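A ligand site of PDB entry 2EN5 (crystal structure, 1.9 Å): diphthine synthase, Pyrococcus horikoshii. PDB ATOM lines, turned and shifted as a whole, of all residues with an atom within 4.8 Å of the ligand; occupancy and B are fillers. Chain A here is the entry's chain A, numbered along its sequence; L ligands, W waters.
Water W2 lies within hydrogen-bond range of an oxygen (O4) of the ligand (2.8 Å) and the backbone carbonyl oxygen (O) of Asp 167 (3.0 Å).
Water W1 lies within hydrogen-bond range of OG1 of Thr 36 (2.7 Å), O of Pro 85 (2.8 Å) and N1 of the ligand (2.9 Å).
The backbone carbonyl oxygen (O) of Leu 166 lies within hydrogen-bond range of an oxygen (O4) of the ligand (2.7 Å).
N of Asp 87 is in hydrogen-bond range of O1 of the ligand.
O of Leu 10 lies within hydrogen-bond range of N4 of the ligand (3.0 Å).
N of Ala 209 lies within hydrogen-bond range of N5 of the ligand, 3.0 Å away.
The backbone carbonyl oxygen of Ala 209 is in hydrogen-bond range of a nitrogen (N4) of the ligand.
The backbone carbonyl oxygen (O) of Val 90 is in hydrogen-bond range of a nitrogen (N1) of the ligand (2.7 Å).
O of Asp 87 lies within hydrogen-bond range of N1 of the ligand (2.7 Å).
O2 of the ligand sits at hydrogen-bond distance from N of Ile 116 (3.0 Å).
An oxygen (O5) of the ligand sits at hydrogen-bond distance from the backbone NH (N) of Leu 166 (2.9 Å).
An oxygen (O1) of the ligand sits at hydrogen-bond distance from the side-chain hydroxyl of Ser 115, at 2.8 Å.
The side-chain hydroxyl of Ser 37 sits close to a nitrogen (N3) of the ligand.
An oxygen (O5) of the ligand is in hydrogen-bond range of the backbone carbonyl oxygen of His 234 (2.7 Å).
O of Thr 36 lies close to S1 of the ligand (3.7 Å).
O of Pro 85 touches N1 of the ligand, 3.9 Å away.
Gly 86 touches the ligand (CA to O1, 3.7 Å).
CB of Ala 91 touches S1 of the ligand, at 3.8 Å.
Thr 92 touches the ligand (CG2 to N1, 3.8 Å).
Phe 165 touches the ligand.
Leu 206 touches the ligand.
N of Arg 208 touches N5 of the ligand, at 3.6 Å.
Pro 233 touches the ligand.
CG2 of Ile 235 touches N6 of the ligand, 3.2 Å away.
Hydrophobic or aromatic side chains within 4 Å of the ligand: Leu 10, Val 90, Ala 91, Ile 116, Phe 165, Leu 166, Ala 209, Pro 233 and Ile 235.
Of the 26 residues printed, 19 come within 4 Å of the ligand.
Along chain A the residues within 4 Å of the ligand span positions 10 to 235.
The nearest printed residue that does not touch the ligand is Asp 167 (4.3 Å).
OG of Ser 115 sits close to N of Tyr 117.
The backbone carbonyl oxygen of Pro 233 is in hydrogen-bond range of the backbone NH of Arg 208, at 3.0 Å.
The backbone NH (N) of Ile 235 sits at hydrogen-bond distance from the backbone carbonyl oxygen (O) of Leu 206 (3.0 Å).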
ATOM      1  N   LEU A  10      -3.040 -19.324  17.827  1.00  0.00           N
ATOM      2  CA  LEU A  10      -2.978 -19.296  19.284  1.00  0.00           C
ATOM      3  C   LEU A  10      -2.655 -18.061  20.107  1.00  0.00           C
ATOM      4  O   LEU A  10      -3.309 -17.797  21.120  1.00  0.00           O
ATOM      5  CB  LEU A  10      -2.003 -20.376  19.744  1.00  0.00           C
ATOM      6  CG  LEU A  10      -2.235 -21.829  19.350  1.00  0.00           C
ATOM      7  CD1 LEU A  10      -0.938 -22.612  19.504  1.00  0.00           C
ATOM      8  CD2 LEU A  10      -3.327 -22.426  20.224  1.00  0.00           C
ATOM      9  N   TYR A  11      -1.644 -17.312  19.699  1.00  0.00           N
ATOM     10  CA  TYR A  11      -1.181 -16.196  20.524  1.00  0.00           C
ATOM     11  C   TYR A  11      -1.035 -14.821  19.876  1.00  0.00           C
ATOM     12  O   TYR A  11      -1.494 -13.824  20.447  1.00  0.00           O
ATOM     13  CB  TYR A  11       0.143 -16.631  21.143  1.00  0.00           C
ATOM     14  CG  TYR A  11       0.753 -15.669  22.128  1.00  0.00           C
ATOM     15  CD1 TYR A  11       0.172 -15.456  23.385  1.00  0.00           C
ATOM     16  CD2 TYR A  11       1.945 -14.997  21.835  1.00  0.00           C
ATOM     17  CE1 TYR A  11       0.752 -14.601  24.315  1.00  0.00           C
ATOM     18  CE2 TYR A  11       2.542 -14.145  22.761  1.00  0.00           C
ATOM     19  CZ  TYR A  11       1.940 -13.948  23.991  1.00  0.00           C
ATOM     20  OH  TYR A  11       2.524 -13.100  24.916  1.00  0.00           O
ATOM     21  N   THR A  36     -14.523 -15.539  21.066  1.00  0.00           N
ATOM     22  CA  THR A  36     -14.427 -16.985  21.294  1.00  0.00           C
ATOM     23  C   THR A  36     -13.126 -17.391  21.986  1.00  0.00           C
ATOM     24  O   THR A  36     -13.022 -18.490  22.525  1.00  0.00           O
ATOM     25  CB  THR A  36     -14.554 -17.795  19.978  1.00  0.00           C
ATOM     26  OG1 THR A  36     -13.574 -17.345  19.034  1.00  0.00           O
ATOM     27  CG2 THR A  36     -15.942 -17.632  19.398  1.00  0.00           C
ATOM     28  N   SER A  37     -12.132 -16.504  21.961  1.00  0.00           N
ATOM     29  CA  SER A  37     -10.858 -16.787  22.611  1.00  0.00           C
ATOM     30  C   SER A  37     -10.049 -15.514  22.754  1.00  0.00           C
ATOM     31  O   SER A  37     -10.469 -14.448  22.309  1.00  0.00           O
ATOM     32  CB  SER A  37     -10.076 -17.830  21.806  1.00  0.00           C
ATOM     33  OG  SER A  37      -8.903 -18.205  22.519  1.00  0.00           O
ATOM     34  N   LEU A  38      -8.876 -15.638  23.359  1.00  0.00           N
ATOM     35  CA  LEU A  38      -8.006 -14.482  23.555  1.00  0.00           C
ATOM     36  C   LEU A  38      -6.612 -14.710  22.974  1.00  0.00           C
ATOM     37  O   LEU A  38      -5.950 -15.693  23.298  1.00  0.00           O
ATOM     38  CB  LEU A  38      -7.871 -14.161  25.056  1.00  0.00           C
ATOM     39  CG  LEU A  38      -6.861 -13.081  25.466  1.00  0.00           C
ATOM     40  CD1 LEU A  38      -7.292 -11.718  24.934  1.00  0.00           C
ATOM     41  CD2 LEU A  38      -6.734 -13.047  26.975  1.00  0.00           C
ATOM     42  N   PRO A  85      -9.826 -16.243  16.411  1.00  0.00           N
ATOM     43  CA  PRO A  85      -8.616 -16.711  17.093  1.00  0.00           C
ATOM     44  C   PRO A  85      -8.539 -18.226  16.877  1.00  0.00           C
ATOM     45  O   PRO A  85      -9.557 -18.857  16.573  1.00  0.00           O
ATOM     46  CB  PRO A  85      -8.894 -16.367  18.568  1.00  0.00           C
ATOM     47  CG  PRO A  85      -9.865 -15.225  18.480  1.00  0.00           C
ATOM     48  CD  PRO A  85     -10.765 -15.626  17.354  1.00  0.00           C
ATOM     49  N   GLY A  86      -7.355 -18.801  17.053  1.00  0.00           N
ATOM     50  CA  GLY A  86      -7.174 -20.245  16.880  1.00  0.00           C
ATOM     51  C   GLY A  86      -7.710 -20.768  15.558  1.00  0.00           C
ATOM     52  O   GLY A  86      -7.486 -20.161  14.508  1.00  0.00           O
ATOM     53  N   ASP A  87      -8.390 -21.918  15.604  1.00  0.00           N
ATOM     54  CA  ASP A  87      -9.000 -22.492  14.415  1.00  0.00           C
ATOM     55  C   ASP A  87     -10.467 -22.097  14.520  1.00  0.00           C
ATOM     56  O   ASP A  87     -11.096 -22.308  15.546  1.00  0.00           O
ATOM     57  CB  ASP A  87      -8.846 -24.014  14.422  1.00  0.00           C
ATOM     58  CG  ASP A  87      -9.496 -24.659  13.213  1.00  0.00           C
ATOM     59  OD1 ASP A  87     -10.740 -24.625  13.103  1.00  0.00           O
ATOM     60  OD2 ASP A  87      -8.755 -25.208  12.357  1.00  0.00           O
ATOM     61  N   VAL A  90     -13.122 -24.859  15.913  1.00  0.00           N
ATOM     62  CA  VAL A  90     -12.849 -25.607  17.134  1.00  0.00           C
ATOM     63  C   VAL A  90     -13.413 -24.966  18.397  1.00  0.00           C
ATOM     64  O   VAL A  90     -13.019 -23.860  18.771  1.00  0.00           O
ATOM     65  CB  VAL A  90     -11.320 -25.823  17.314  1.00  0.00           C
ATOM     66  CG1 VAL A  90     -11.035 -26.473  18.664  1.00  0.00           C
ATOM     67  CG2 VAL A  90     -10.793 -26.703  16.173  1.00  0.00           C
ATOM     68  N   ALA A  91     -14.325 -25.670  19.062  1.00  0.00           N
ATOM     69  CA  ALA A  91     -14.925 -25.171  20.296  1.00  0.00           C
ATOM     70  C   ALA A  91     -15.652 -23.845  20.095  1.00  0.00           C
ATOM     71  O   ALA A  91     -15.629 -22.966  20.957  1.00  0.00           O
ATOM     72  CB  ALA A  91     -13.865 -25.037  21.382  1.00  0.00           C
ATOM     73  N   THR A  92     -16.269 -23.705  18.921  1.00  0.00           N
ATOM     74  CA  THR A  92     -17.062 -22.531  18.576  1.00  0.00           C
ATOM     75  C   THR A  92     -18.264 -23.131  17.874  1.00  0.00           C
ATOM     76  O   THR A  92     -18.314 -24.340  17.647  1.00  0.00           O
ATOM     77  CB  THR A  92     -16.336 -21.596  17.565  1.00  0.00           C
ATOM     78  OG1 THR A  92     -16.260 -22.245  16.287  1.00  0.00           O
ATOM     79  CG2 THR A  92     -14.923 -21.274  18.041  1.00  0.00           C
ATOM     80  N   PRO A 114      -3.186 -22.981  14.007  1.00  0.00           N
ATOM     81  CA  PRO A 114      -2.952 -23.751  15.234  1.00  0.00           C
ATOM     82  C   PRO A 114      -4.082 -23.534  16.237  1.00  0.00           C
ATOM     83  O   PRO A 114      -4.576 -22.420  16.425  1.00  0.00           O
ATOM     84  CB  PRO A 114      -1.588 -23.247  15.719  1.00  0.00           C
ATOM     85  CG  PRO A 114      -1.401 -21.927  15.030  1.00  0.00           C
ATOM     86  CD  PRO A 114      -2.024 -22.135  13.674  1.00  0.00           C
ATOM     87  N   SER A 115      -4.493 -24.634  16.861  1.00  0.00           N
ATOM     88  CA  SER A 115      -5.596 -24.650  17.821  1.00  0.00           C
ATOM     89  C   SER A 115      -5.141 -25.146  19.198  1.00  0.00           C
ATOM     90  O   SER A 115      -4.250 -25.978  19.300  1.00  0.00           O
ATOM     91  CB  SER A 115      -6.702 -25.575  17.301  1.00  0.00           C
ATOM     92  OG  SER A 115      -7.702 -25.806  18.277  1.00  0.00           O
ATOM     93  N   ILE A 116      -5.768 -24.631  20.246  1.00  0.00           N
ATOM     94  CA  ILE A 116      -5.418 -25.069  21.584  1.00  0.00           C
ATOM     95  C   ILE A 116      -5.693 -26.575  21.708  1.00  0.00           C
ATOM     96  O   ILE A 116      -5.042 -27.274  22.490  1.00  0.00           O
ATOM     97  CB  ILE A 116      -6.234 -24.311  22.668  1.00  0.00           C
ATOM     98  CG1 ILE A 116      -5.719 -24.683  24.058  1.00  0.00           C
ATOM     99  CG2 ILE A 116      -7.725 -24.655  22.553  1.00  0.00           C
ATOM    100  CD1 ILE A 116      -4.273 -24.295  24.301  1.00  0.00           C
ATOM    101  N   TYR A 117      -6.628 -27.083  20.907  1.00  0.00           N
ATOM    102  CA  TYR A 117      -6.969 -28.501  20.977  1.00  0.00           C
ATOM    103  C   TYR A 117      -5.795 -29.424  20.643  1.00  0.00           C
ATOM    104  O   TYR A 117      -5.652 -30.491  21.236  1.00  0.00           O
ATOM    105  CB  TYR A 117      -8.160 -28.801  20.052  1.00  0.00           C
ATOM    106  CG  TYR A 117      -8.799 -30.152  20.309  1.00  0.00           C
ATOM    107  CD1 TYR A 117      -9.496 -30.403  21.492  1.00  0.00           C
ATOM    108  CD2 TYR A 117      -8.704 -31.178  19.362  1.00  0.00           C
ATOM    109  CE1 TYR A 117     -10.078 -31.649  21.733  1.00  0.00           C
ATOM    110  CE2 TYR A 117      -9.276 -32.425  19.592  1.00  0.00           C
ATOM    111  CZ  TYR A 117      -9.956 -32.658  20.779  1.00  0.00           C
ATOM    112  OH  TYR A 117     -10.516 -33.892  21.000  1.00  0.00           O
ATOM    113  N   PHE A 165     -11.637 -26.506  28.550  1.00  0.00           N
ATOM    114  CA  PHE A 165     -11.567 -25.158  28.000  1.00  0.00           C
ATOM    115  C   PHE A 165     -12.079 -24.303  29.149  1.00  0.00           C
ATOM    116  O   PHE A 165     -12.959 -24.744  29.892  1.00  0.00           O
ATOM    117  CB  PHE A 165     -12.536 -24.987  26.828  1.00  0.00           C
ATOM    118  CG  PHE A 165     -12.210 -25.833  25.638  1.00  0.00           C
ATOM    119  CD1 PHE A 165     -11.201 -25.450  24.750  1.00  0.00           C
ATOM    120  CD2 PHE A 165     -12.920 -27.009  25.391  1.00  0.00           C
ATOM    121  CE1 PHE A 165     -10.913 -26.229  23.643  1.00  0.00           C
ATOM    122  CE2 PHE A 165     -12.628 -27.796  24.279  1.00  0.00           C
ATOM    123  CZ  PHE A 165     -11.627 -27.398  23.402  1.00  0.00           C
ATOM    124  N   LEU A 166     -11.554 -23.093  29.302  1.00  0.00           N
ATOM    125  CA  LEU A 166     -12.014 -22.222  30.389  1.00  0.00           C
ATOM    126  C   LEU A 166     -12.882 -21.086  29.849  1.00  0.00           C
ATOM    127  O   LEU A 166     -12.715 -20.643  28.713  1.00  0.00           O
ATOM    128  CB  LEU A 166     -10.803 -21.693  31.178  1.00  0.00           C
ATOM    129  CG  LEU A 166      -9.894 -22.802  31.726  1.00  0.00           C
ATOM    130  CD1 LEU A 166      -8.840 -22.187  32.637  1.00  0.00           C
ATOM    131  CD2 LEU A 166     -10.695 -23.837  32.498  1.00  0.00           C
ATOM    132  N   ASP A 167     -13.819 -20.634  30.675  1.00  0.00           N
ATOM    133  CA  ASP A 167     -14.764 -19.586  30.277  1.00  0.00           C
ATOM    134  C   ASP A 167     -14.141 -18.253  29.888  1.00  0.00           C
ATOM    135  O   ASP A 167     -13.026 -17.905  30.281  1.00  0.00           O
ATOM    136  CB  ASP A 167     -15.794 -19.366  31.397  1.00  0.00           C
ATOM    137  CG  ASP A 167     -17.168 -19.007  30.867  1.00  0.00           C
ATOM    138  OD1 ASP A 167     -17.287 -18.707  29.651  1.00  0.00           O
ATOM    139  OD2 ASP A 167     -18.129 -19.018  31.657  1.00  0.00           O
ATOM    140  N   ILE A 168     -14.906 -17.489  29.108  1.00  0.00           N
ATOM    141  CA  ILE A 168     -14.491 -16.176  28.649  1.00  0.00           C
ATOM    142  C   ILE A 168     -15.713 -15.282  28.447  1.00  0.00           C
ATOM    143  O   ILE A 168     -16.714 -15.682  27.855  1.00  0.00           O
ATOM    144  CB  ILE A 168     -13.701 -16.272  27.312  1.00  0.00           C
ATOM    145  CG1 ILE A 168     -13.437 -14.867  26.755  1.00  0.00           C
ATOM    146  CG2 ILE A 168     -14.461 -17.118  26.306  1.00  0.00           C
ATOM    147  CD1 ILE A 168     -12.553 -14.850  25.525  1.00  0.00           C
ATOM    148  N   LEU A 206      -1.761 -25.076  31.128  1.00  0.00           N
ATOM    149  CA  LEU A 206      -1.065 -24.565  29.952  1.00  0.00           C
ATOM    150  C   LEU A 206      -1.596 -23.160  29.733  1.00  0.00           C
ATOM    151  O   LEU A 206      -2.789 -22.955  29.515  1.00  0.00           O
ATOM    152  CB  LEU A 206      -1.366 -25.441  28.723  1.00  0.00           C
ATOM    153  CG  LEU A 206      -0.808 -24.930  27.384  1.00  0.00           C
ATOM    154  CD1 LEU A 206       0.706 -24.712  27.487  1.00  0.00           C
ATOM    155  CD2 LEU A 206      -1.122 -25.941  26.277  1.00  0.00           C
ATOM    156  N   ALA A 207      -0.702 -22.183  29.846  1.00  0.00           N
ATOM    157  CA  ALA A 207      -1.081 -20.780  29.675  1.00  0.00           C
ATOM    158  C   ALA A 207      -0.348 -20.127  28.528  1.00  0.00           C
ATOM    159  O   ALA A 207       0.861 -20.283  28.382  1.00  0.00           O
ATOM    160  CB  ALA A 207      -0.810 -20.004  30.967  1.00  0.00           C
ATOM    161  N   ARG A 208      -1.096 -19.380  27.726  1.00  0.00           N
ATOM    162  CA  ARG A 208      -0.560 -18.660  26.578  1.00  0.00           C
ATOM    163  C   ARG A 208       0.209 -19.553  25.593  1.00  0.00           C
ATOM    164  O   ARG A 208       1.341 -19.262  25.220  1.00  0.00           O
ATOM    165  CB  ARG A 208       0.329 -17.511  27.070  1.00  0.00           C
ATOM    166  CG  ARG A 208      -0.403 -16.568  28.044  1.00  0.00           C
ATOM    167  CD  ARG A 208       0.528 -15.481  28.594  1.00  0.00           C
ATOM    168  NE  ARG A 208       1.776 -16.052  29.097  1.00  0.00           N
ATOM    169  CZ  ARG A 208       1.883 -16.756  30.222  1.00  0.00           C
ATOM    170  NH1 ARG A 208       0.808 -16.974  30.987  1.00  0.00           N
ATOM    171  NH2 ARG A 208       3.052 -17.280  30.556  1.00  0.00           N
ATOM    172  N   ALA A 209      -0.427 -20.647  25.192  1.00  0.00           N
ATOM    173  CA  ALA A 209       0.175 -21.545  24.215  1.00  0.00           C
ATOM    174  C   ALA A 209       0.341 -20.704  22.951  1.00  0.00           C
ATOM    175  O   ALA A 209      -0.472 -19.819  22.681  1.00  0.00           O
ATOM    176  CB  ALA A 209      -0.742 -22.731  23.957  1.00  0.00           C
ATOM    177  N   PRO A 233      -4.805 -16.398  27.989  1.00  0.00           N
ATOM    178  CA  PRO A 233      -5.705 -17.495  28.328  1.00  0.00           C
ATOM    179  C   PRO A 233      -5.028 -18.716  28.951  1.00  0.00           C
ATOM    180  O   PRO A 233      -3.826 -18.940  28.767  1.00  0.00           O
ATOM    181  CB  PRO A 233      -6.343 -17.824  26.984  1.00  0.00           C
ATOM    182  CG  PRO A 233      -5.192 -17.631  26.049  1.00  0.00           C
ATOM    183  CD  PRO A 233      -4.571 -16.337  26.531  1.00  0.00           C
ATOM    184  N   HIS A 234      -5.817 -19.484  29.694  1.00  0.00           N
ATOM    185  CA  HIS A 234      -5.356 -20.709  30.346  1.00  0.00           C
ATOM    186  C   HIS A 234      -6.295 -21.849  29.992  1.00  0.00           C
ATOM    187  O   HIS A 234      -7.459 -21.629  29.662  1.00  0.00           O
ATOM    188  CB  HIS A 234      -5.443 -20.601  31.886  1.00  0.00           C
ATOM    189  CG  HIS A 234      -4.571 -19.550  32.501  1.00  0.00           C
ATOM    190  ND1 HIS A 234      -4.538 -19.345  33.859  1.00  0.00           N
ATOM    191  CD2 HIS A 234      -3.713 -18.649  31.967  1.00  0.00           C
ATOM    192  CE1 HIS A 234      -3.696 -18.369  34.139  1.00  0.00           C
ATOM    193  NE2 HIS A 234      -3.185 -17.934  33.001  1.00  0.00           N
ATOM    194  N   ILE A 235      -5.774 -23.072  30.081  1.00  0.00           N
ATOM    195  CA  ILE A 235      -6.609 -24.258  29.913  1.00  0.00           C
ATOM    196  C   ILE A 235      -6.171 -25.142  31.064  1.00  0.00           C
ATOM    197  O   ILE A 235      -5.037 -25.041  31.534  1.00  0.00           O
ATOM    198  CB  ILE A 235      -6.396 -25.060  28.588  1.00  0.00           C
ATOM    199  CG1 ILE A 235      -4.920 -25.415  28.398  1.00  0.00           C
ATOM    200  CG2 ILE A 235      -6.961 -24.289  27.437  1.00  0.00           C
ATOM    201  CD1 ILE A 235      -4.726 -26.590  27.445  1.00  0.00           C
HETATM  202  N1  LIG L   1     -11.192 -21.997  18.256  1.00  0.00           N
HETATM  203  C1  LIG L   1     -10.246 -21.847  19.446  1.00  0.00           C
HETATM  204  C2  LIG L   1     -10.777 -22.241  20.787  1.00  0.00           C
HETATM  205  C3  LIG L   1     -12.033 -21.544  21.305  1.00  0.00           C
HETATM  206  S1  LIG L   1     -12.233 -22.013  23.072  1.00  0.00           S
HETATM  207  C4  LIG L   1      -8.948 -22.677  19.083  1.00  0.00           C
HETATM  208  O1  LIG L   1      -8.902 -23.289  17.989  1.00  0.00           O
HETATM  209  O2  LIG L   1      -7.987 -22.677  19.961  1.00  0.00           O
HETATM  210  C5  LIG L   1     -11.296 -20.738  23.821  1.00  0.00           C
HETATM  211  C6  LIG L   1     -10.664 -21.273  25.167  1.00  0.00           C
HETATM  212  O3  LIG L   1      -9.605 -22.194  24.791  1.00  0.00           O
HETATM  213  C7  LIG L   1     -10.028 -20.237  26.029  1.00  0.00           C
HETATM  214  O4  LIG L   1     -10.976 -19.671  26.910  1.00  0.00           O
HETATM  215  C8  LIG L   1      -8.900 -21.048  26.693  1.00  0.00           C
HETATM  216  O5  LIG L   1      -9.372 -21.793  27.827  1.00  0.00           O
HETATM  217  C9  LIG L   1      -8.361 -21.923  25.554  1.00  0.00           C
HETATM  218  N2  LIG L   1      -7.423 -21.338  24.760  1.00  0.00           N
HETATM  219  C10 LIG L   1      -7.435 -20.739  23.512  1.00  0.00           C
HETATM  220  N3  LIG L   1      -6.292 -20.303  23.093  1.00  0.00           N
HETATM  221  C11 LIG L   1      -5.396 -20.618  24.143  1.00  0.00           C
HETATM  222  C12 LIG L   1      -3.974 -20.392  24.284  1.00  0.00           C
HETATM  223  N4  LIG L   1      -3.218 -19.786  23.362  1.00  0.00           N
HETATM  224  N5  LIG L   1      -3.430 -20.850  25.465  1.00  0.00           N
HETATM  225  C13 LIG L   1      -4.161 -21.464  26.433  1.00  0.00           C
HETATM  226  N6  LIG L   1      -5.514 -21.691  26.338  1.00  0.00           N
HETATM  227  C14 LIG L   1      -6.063 -21.247  25.173  1.00  0.00           C
HETATM  228  O   HOH W   1     -11.806 -19.199  18.272  1.00  0.00           O
HETATM  229  O   HOH W   2     -10.470 -17.602  28.726  1.00  0.00           O
HETATM  230  O   HOH W   3      -6.563 -20.214  20.306  1.00  0.00           O
HETATM  231  O   HOH W   4      -6.666 -17.703  21.046  1.00  0.00           O
